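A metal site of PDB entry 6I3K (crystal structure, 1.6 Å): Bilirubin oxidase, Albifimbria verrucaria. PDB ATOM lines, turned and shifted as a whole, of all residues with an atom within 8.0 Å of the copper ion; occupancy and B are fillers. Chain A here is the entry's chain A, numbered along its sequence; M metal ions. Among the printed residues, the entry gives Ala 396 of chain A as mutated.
The copper ion is bound by a ring nitrogen (ND1) of His 398 (2.0 Å), a ring nitrogen (ND1) of His 462 (2.0 Å) and the side-chain sulfur (SG) of Cys 457 (2.2 Å). The copper ion has three donor atoms within binding distance.
Thr 397 touches the copper ion (O to CU, 3.5 Å). Met 467 touches the copper ion. The nearest printed residue that does not touch the copper ion is Asn 459 (4.03 Å).
The backbone NH (N) of Cys 457 lies within hydrogen-bond range of the backbone carbonyl oxygen (O) of Met 467. N of Met 467 is in hydrogen-bond range of O of His 462, at 2.9 Å. N of Asn 459 lies close to SG of Cys 457 (3.4 Å). OG1 of Thr 397 is in hydrogen-bond range of NE1 of Trp 433 (3.0 Å). A ring nitrogen (ND1) of His 398 sits close to the side-chain sulfur of Met 467. The backbone carbonyl oxygen of Trp 361 lies within hydrogen-bond range of the backbone NH of Met 467, at 3.2 Å. The side-chain amide oxygen of Asn 459 is in hydrogen-bond range of the backbone NH of His 462. The backbone carbonyl oxygen of Asn 197 is in hydrogen-bond range of a ring nitrogen (NE2) of His 462, 3.0 Å away.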
ATOM      1  N   ASN A 197      19.011 -11.439  15.679  1.00  0.00           N
ATOM      2  CA  ASN A 197      19.085 -10.945  14.275  1.00  0.00           C
ATOM      3  C   ASN A 197      18.934 -12.124  13.293  1.00  0.00           C
ATOM      4  O   ASN A 197      17.906 -12.235  12.636  1.00  0.00           O
ATOM      5  CB  ASN A 197      20.397 -10.211  13.958  1.00  0.00           C
ATOM      6  CG  ASN A 197      20.440  -9.635  12.556  1.00  0.00           C
ATOM      7  OD1 ASN A 197      19.453  -9.036  12.083  1.00  0.00           O
ATOM      8  ND2 ASN A 197      21.596  -9.775  11.898  1.00  0.00           N
ATOM      9  N   SER A 198      19.967 -12.962  13.201  1.00  0.00           N
ATOM     10  CA  SER A 198      20.027 -14.169  12.342  1.00  0.00           C
ATOM     11  C   SER A 198      21.232 -14.963  12.763  1.00  0.00           C
ATOM     12  O   SER A 198      22.217 -14.335  13.199  1.00  0.00           O
ATOM     13  CB  SER A 198      20.093 -13.858  10.848  1.00  0.00           C
ATOM     14  OG  SER A 198      18.854 -13.548  10.267  1.00  0.00           O
ATOM     15  N   MET A 273      14.877 -20.663   3.520  1.00  0.00           N
ATOM     16  CA  MET A 273      14.525 -21.579   4.615  1.00  0.00           C
ATOM     17  C   MET A 273      13.116 -22.169   4.399  1.00  0.00           C
ATOM     18  O   MET A 273      12.156 -21.420   4.175  1.00  0.00           O
ATOM     19  CB  MET A 273      14.570 -20.903   5.989  1.00  0.00           C
ATOM     20  CG  MET A 273      15.982 -20.551   6.459  1.00  0.00           C
ATOM     21  SD  MET A 273      16.798 -19.179   5.591  1.00  0.00           S
ATOM     22  CE  MET A 273      15.979 -17.735   6.252  1.00  0.00           C
ATOM     23  N   PHE A 354       6.094  -7.404   6.912  1.00  0.00           N
ATOM     24  CA  PHE A 354       7.129  -8.119   7.677  1.00  0.00           C
ATOM     25  C   PHE A 354       8.225  -7.094   7.982  1.00  0.00           C
ATOM     26  O   PHE A 354       8.954  -6.661   7.042  1.00  0.00           O
ATOM     27  CB  PHE A 354       7.566  -9.306   6.837  1.00  0.00           C
ATOM     28  CG  PHE A 354       6.437 -10.273   6.602  1.00  0.00           C
ATOM     29  CD1 PHE A 354       6.176 -11.263   7.543  1.00  0.00           C
ATOM     30  CD2 PHE A 354       5.600 -10.169   5.514  1.00  0.00           C
ATOM     31  CE1 PHE A 354       5.119 -12.151   7.375  1.00  0.00           C
ATOM     32  CE2 PHE A 354       4.521 -11.038   5.369  1.00  0.00           C
ATOM     33  CZ  PHE A 354       4.278 -12.018   6.304  1.00  0.00           C
ATOM     34  N   GLY A 355       8.329  -6.706   9.230  1.00  0.00           N
ATOM     35  CA  GLY A 355       9.353  -5.727   9.639  1.00  0.00           C
ATOM     36  C   GLY A 355       9.644  -5.838  11.123  1.00  0.00           C
ATOM     37  O   GLY A 355       9.542  -6.926  11.660  1.00  0.00           O
ATOM     38  N   TRP A 361      10.911  -8.803  15.600  1.00  0.00           N
ATOM     39  CA  TRP A 361      10.381  -9.133  14.252  1.00  0.00           C
ATOM     40  C   TRP A 361       8.883  -9.379  14.316  1.00  0.00           C
ATOM     41  O   TRP A 361       8.506 -10.250  15.122  1.00  0.00           O
ATOM     42  CB  TRP A 361      11.187 -10.315  13.687  1.00  0.00           C
ATOM     43  CG  TRP A 361      12.666 -10.074  13.637  1.00  0.00           C
ATOM     44  CD1 TRP A 361      13.590 -10.548  14.511  1.00  0.00           C
ATOM     45  CD2 TRP A 361      13.411  -9.347  12.624  1.00  0.00           C
ATOM     46  NE1 TRP A 361      14.857 -10.153  14.127  1.00  0.00           N
ATOM     47  CE2 TRP A 361      14.767  -9.413  12.986  1.00  0.00           C
ATOM     48  CE3 TRP A 361      13.049  -8.681  11.456  1.00  0.00           C
ATOM     49  CZ2 TRP A 361      15.776  -8.833  12.206  1.00  0.00           C
ATOM     50  CZ3 TRP A 361      14.046  -8.063  10.698  1.00  0.00           C
ATOM     51  CH2 TRP A 361      15.377  -8.128  11.095  1.00  0.00           C
ATOM     52  N   THR A 362       8.079  -8.621  13.550  1.00  0.00           N
ATOM     53  CA  THR A 362       6.611  -8.565  13.672  1.00  0.00           C
ATOM     54  C   THR A 362       5.932  -8.673  12.322  1.00  0.00           C
ATOM     55  O   THR A 362       6.581  -8.515  11.268  1.00  0.00           O
ATOM     56  CB  THR A 362       6.176  -7.295  14.428  1.00  0.00           C
ATOM     57  OG1 THR A 362       6.706  -6.133  13.776  1.00  0.00           O
ATOM     58  CG2 THR A 362       6.607  -7.335  15.877  1.00  0.00           C
ATOM     59  N   ASN A 391       7.996  -6.979   2.216  1.00  0.00           N
ATOM     60  CA  ASN A 391       9.245  -6.704   2.934  1.00  0.00           C
ATOM     61  C   ASN A 391       9.677  -5.287   2.504  1.00  0.00           C
ATOM     62  O   ASN A 391      10.320  -5.172   1.444  1.00  0.00           O
ATOM     63  CB  ASN A 391      10.357  -7.688   2.592  1.00  0.00           C
ATOM     64  CG  ASN A 391      11.663  -7.384   3.291  1.00  0.00           C
ATOM     65  OD1 ASN A 391      11.630  -6.710   4.333  1.00  0.00           O
ATOM     66  ND2 ASN A 391      12.774  -7.959   2.819  1.00  0.00           N
ATOM     67  N   ALA A 396      17.046  -6.986   5.873  1.00  0.00           N
ATOM     68  CA  ALA A 396      16.755  -8.401   6.147  1.00  0.00           C
ATOM     69  C   ALA A 396      15.869  -8.967   5.043  1.00  0.00           C
ATOM     70  O   ALA A 396      15.269  -8.178   4.273  1.00  0.00           O
ATOM     71  CB  ALA A 396      16.081  -8.520   7.478  1.00  0.00           C
ATOM     72  N   THR A 397      15.748 -10.303   5.019  1.00  0.00           N
ATOM     73  CA  THR A 397      14.839 -10.999   4.093  1.00  0.00           C
ATOM     74  C   THR A 397      14.043 -12.036   4.871  1.00  0.00           C
ATOM     75  O   THR A 397      14.451 -12.478   5.918  1.00  0.00           O
ATOM     76  CB  THR A 397      15.598 -11.661   2.938  1.00  0.00           C
ATOM     77  OG1 THR A 397      16.328 -12.809   3.390  1.00  0.00           O
ATOM     78  CG2 THR A 397      16.546 -10.694   2.262  1.00  0.00           C
ATOM     79  N   HIS A 398      12.935 -12.464   4.265  1.00  0.00           N
ATOM     80  CA  HIS A 398      11.887 -13.223   5.012  1.00  0.00           C
ATOM     81  C   HIS A 398      11.276 -14.246   4.055  1.00  0.00           C
ATOM     82  O   HIS A 398      10.462 -13.873   3.194  1.00  0.00           O
ATOM     83  CB  HIS A 398      10.819 -12.255   5.562  1.00  0.00           C
ATOM     84  CG  HIS A 398      11.374 -11.089   6.318  1.00  0.00           C
ATOM     85  ND1 HIS A 398      11.986 -11.289   7.542  1.00  0.00           N
ATOM     86  CD2 HIS A 398      11.510  -9.794   5.991  1.00  0.00           C
ATOM     87  CE1 HIS A 398      12.401 -10.108   7.965  1.00  0.00           C
ATOM     88  NE2 HIS A 398      12.142  -9.169   7.034  1.00  0.00           N
ATOM     89  N   PRO A 399      11.586 -15.545   4.212  1.00  0.00           N
ATOM     90  CA  PRO A 399      10.844 -16.610   3.527  1.00  0.00           C
ATOM     91  C   PRO A 399       9.530 -16.870   4.281  1.00  0.00           C
ATOM     92  O   PRO A 399       9.540 -17.391   5.387  1.00  0.00           O
ATOM     93  CB  PRO A 399      11.821 -17.785   3.525  1.00  0.00           C
ATOM     94  CG  PRO A 399      12.646 -17.593   4.783  1.00  0.00           C
ATOM     95  CD  PRO A 399      12.719 -16.098   4.987  1.00  0.00           C
ATOM     96  N   ILE A 400       8.415 -16.468   3.674  1.00  0.00           N
ATOM     97  CA  ILE A 400       7.083 -16.537   4.316  1.00  0.00           C
ATOM     98  C   ILE A 400       6.408 -17.886   4.031  1.00  0.00           C
ATOM     99  O   ILE A 400       6.271 -18.294   2.845  1.00  0.00           O
ATOM    100  CB  ILE A 400       6.199 -15.368   3.895  1.00  0.00           C
ATOM    101  CG1 ILE A 400       6.911 -14.040   4.147  1.00  0.00           C
ATOM    102  CG2 ILE A 400       4.852 -15.452   4.621  1.00  0.00           C
ATOM    103  CD1 ILE A 400       7.494 -13.882   5.509  1.00  0.00           C
ATOM    104  N   TRP A 433      10.163 -16.584  -0.899  1.00  0.00           N
ATOM    105  CA  TRP A 433      11.261 -15.738  -0.357  1.00  0.00           C
ATOM    106  C   TRP A 433      11.030 -14.261  -0.687  1.00  0.00           C
ATOM    107  O   TRP A 433      11.054 -13.891  -1.893  1.00  0.00           O
ATOM    108  CB  TRP A 433      12.593 -16.190  -0.887  1.00  0.00           C
ATOM    109  CG  TRP A 433      13.771 -15.540  -0.216  1.00  0.00           C
ATOM    110  CD1 TRP A 433      13.837 -14.977   1.017  1.00  0.00           C
ATOM    111  CD2 TRP A 433      15.122 -15.605  -0.701  1.00  0.00           C
ATOM    112  NE1 TRP A 433      15.129 -14.583   1.296  1.00  0.00           N
ATOM    113  CE2 TRP A 433      15.936 -14.958   0.257  1.00  0.00           C
ATOM    114  CE3 TRP A 433      15.693 -16.052  -1.891  1.00  0.00           C
ATOM    115  CZ2 TRP A 433      17.309 -14.768   0.082  1.00  0.00           C
ATOM    116  CZ3 TRP A 433      17.062 -15.910  -2.057  1.00  0.00           C
ATOM    117  CH2 TRP A 433      17.843 -15.270  -1.082  1.00  0.00           C
ATOM    118  N   LEU A 434      10.826 -13.434   0.353  1.00  0.00           N
ATOM    119  CA  LEU A 434      10.838 -11.955   0.224  1.00  0.00           C
ATOM    120  C   LEU A 434      12.279 -11.500   0.401  1.00  0.00           C
ATOM    121  O   LEU A 434      12.735 -11.290   1.539  1.00  0.00           O
ATOM    122  CB  LEU A 434       9.924 -11.260   1.241  1.00  0.00           C
ATOM    123  CG  LEU A 434       8.497 -11.775   1.364  1.00  0.00           C
ATOM    124  CD1 LEU A 434       7.758 -10.913   2.378  1.00  0.00           C
ATOM    125  CD2 LEU A 434       7.777 -11.785   0.029  1.00  0.00           C
ATOM    126  N   HIS A 456       4.030 -17.305   9.019  1.00  0.00           N
ATOM    127  CA  HIS A 456       5.237 -16.743   9.655  1.00  0.00           C
ATOM    128  C   HIS A 456       6.373 -16.648   8.659  1.00  0.00           C
ATOM    129  O   HIS A 456       6.391 -17.344   7.632  1.00  0.00           O
ATOM    130  CB  HIS A 456       5.677 -17.588  10.854  1.00  0.00           C
ATOM    131  CG  HIS A 456       5.934 -19.042  10.567  1.00  0.00           C
ATOM    132  ND1 HIS A 456       7.186 -19.538  10.422  1.00  0.00           N
ATOM    133  CD2 HIS A 456       5.101 -20.108  10.482  1.00  0.00           C
ATOM    134  CE1 HIS A 456       7.134 -20.858  10.327  1.00  0.00           C
ATOM    135  NE2 HIS A 456       5.863 -21.232  10.305  1.00  0.00           N
ATOM    136  N   CYS A 457       7.348 -15.821   9.002  1.00  0.00           N
ATOM    137  CA  CYS A 457       8.704 -15.955   8.443  1.00  0.00           C
ATOM    138  C   CYS A 457       9.310 -17.289   8.926  1.00  0.00           C
ATOM    139  O   CYS A 457       9.200 -17.594  10.134  1.00  0.00           O
ATOM    140  CB  CYS A 457       9.560 -14.774   8.841  1.00  0.00           C
ATOM    141  SG  CYS A 457      11.235 -14.911   8.205  1.00  0.00           S
ATOM    142  N   HIS A 458      10.016 -18.017   8.050  1.00  0.00           N
ATOM    143  CA  HIS A 458      10.671 -19.286   8.390  1.00  0.00           C
ATOM    144  C   HIS A 458      12.182 -19.135   8.613  1.00  0.00           C
ATOM    145  O   HIS A 458      12.874 -20.177   8.768  1.00  0.00           O
ATOM    146  CB  HIS A 458      10.292 -20.360   7.340  1.00  0.00           C
ATOM    147  CG  HIS A 458      10.079 -21.732   7.903  1.00  0.00           C
ATOM    148  ND1 HIS A 458      11.054 -22.452   8.536  1.00  0.00           N
ATOM    149  CD2 HIS A 458       8.997 -22.532   7.856  1.00  0.00           C
ATOM    150  CE1 HIS A 458      10.563 -23.633   8.896  1.00  0.00           C
ATOM    151  NE2 HIS A 458       9.313 -23.704   8.450  1.00  0.00           N
ATOM    152  N   ASN A 459      12.730 -17.905   8.673  1.00  0.00           N
ATOM    153  CA  ASN A 459      14.019 -17.669   9.358  1.00  0.00           C
ATOM    154  C   ASN A 459      13.762 -17.931  10.863  1.00  0.00           C
ATOM    155  O   ASN A 459      12.927 -17.186  11.442  1.00  0.00           O
ATOM    156  CB  ASN A 459      14.502 -16.237   9.127  1.00  0.00           C
ATOM    157  CG  ASN A 459      15.833 -15.945   9.773  1.00  0.00           C
ATOM    158  OD1 ASN A 459      16.084 -16.392  10.893  1.00  0.00           O
ATOM    159  ND2 ASN A 459      16.666 -15.137   9.073  1.00  0.00           N
ATOM    160  N   LEU A 460      14.344 -18.976  11.410  1.00  0.00           N
ATOM    161  CA  LEU A 460      13.861 -19.491  12.720  1.00  0.00           C
ATOM    162  C   LEU A 460      14.181 -18.454  13.819  1.00  0.00           C
ATOM    163  O   LEU A 460      13.430 -18.403  14.820  1.00  0.00           O
ATOM    164  CB  LEU A 460      14.434 -20.866  13.047  1.00  0.00           C
ATOM    165  CG  LEU A 460      14.183 -21.941  11.965  1.00  0.00           C
ATOM    166  CD1 LEU A 460      14.764 -23.263  12.439  1.00  0.00           C
ATOM    167  CD2 LEU A 460      12.718 -22.135  11.626  1.00  0.00           C
ATOM    168  N   ILE A 461      15.212 -17.627  13.625  1.00  0.00           N
ATOM    169  CA  ILE A 461      15.511 -16.528  14.607  1.00  0.00           C
ATOM    170  C   ILE A 461      14.395 -15.494  14.545  1.00  0.00           C
ATOM    171  O   ILE A 461      13.874 -15.112  15.610  1.00  0.00           O
ATOM    172  CB  ILE A 461      16.881 -15.895  14.350  1.00  0.00           C
ATOM    173  CG1 ILE A 461      18.026 -16.894  14.473  1.00  0.00           C
ATOM    174  CG2 ILE A 461      17.073 -14.670  15.214  1.00  0.00           C
ATOM    175  CD1 ILE A 461      18.150 -17.541  15.867  1.00  0.00           C
ATOM    176  N   HIS A 462      13.983 -15.051  13.350  1.00  0.00           N
ATOM    177  CA  HIS A 462      12.865 -14.093  13.195  1.00  0.00           C
ATOM    178  C   HIS A 462      11.586 -14.699  13.815  1.00  0.00           C
ATOM    179  O   HIS A 462      10.879 -13.993  14.536  1.00  0.00           O
ATOM    180  CB  HIS A 462      12.646 -13.690  11.739  1.00  0.00           C
ATOM    181  CG  HIS A 462      13.827 -12.999  11.117  1.00  0.00           C
ATOM    182  ND1 HIS A 462      13.766 -12.627   9.761  1.00  0.00           N
ATOM    183  CD2 HIS A 462      15.020 -12.592  11.618  1.00  0.00           C
ATOM    184  CE1 HIS A 462      14.930 -12.049   9.452  1.00  0.00           C
ATOM    185  NE2 HIS A 462      15.706 -11.978  10.585  1.00  0.00           N
ATOM    186  N   GLU A 463      11.302 -15.947  13.456  1.00  0.00           N
ATOM    187  CA  GLU A 463      10.106 -16.699  13.911  1.00  0.00           C
ATOM    188  C   GLU A 463      10.011 -16.686  15.432  1.00  0.00           C
ATOM    189  O   GLU A 463       8.916 -16.426  15.957  1.00  0.00           O
ATOM    190  CB  GLU A 463      10.238 -18.130  13.360  1.00  0.00           C
ATOM    191  CG  GLU A 463       9.082 -19.050  13.739  1.00  0.00           C
ATOM    192  CD  GLU A 463       9.151 -20.404  13.046  1.00  0.00           C
ATOM    193  OE1 GLU A 463       9.750 -20.486  11.942  1.00  0.00           O
ATOM    194  OE2 GLU A 463       8.628 -21.393  13.650  1.00  0.00           O
ATOM    195  N   MET A 467       8.086 -13.380  14.732  1.00  0.00           N
ATOM    196  CA  MET A 467       7.476 -12.948  13.455  1.00  0.00           C
ATOM    197  C   MET A 467       6.541 -14.055  12.955  1.00  0.00           C
ATOM    198  O   MET A 467       6.817 -14.755  11.950  1.00  0.00           O
ATOM    199  CB  MET A 467       8.585 -12.634  12.437  1.00  0.00           C
ATOM    200  CG  MET A 467       8.088 -11.996  11.188  1.00  0.00           C
ATOM    201  SD  MET A 467       9.439 -11.612  10.016  1.00  0.00           S
ATOM    202  CE  MET A 467       9.508  -9.823  10.108  1.00  0.00           C
HETATM  203 CU    CU M   1      12.216 -12.973   8.558  1.00  0.00          CU
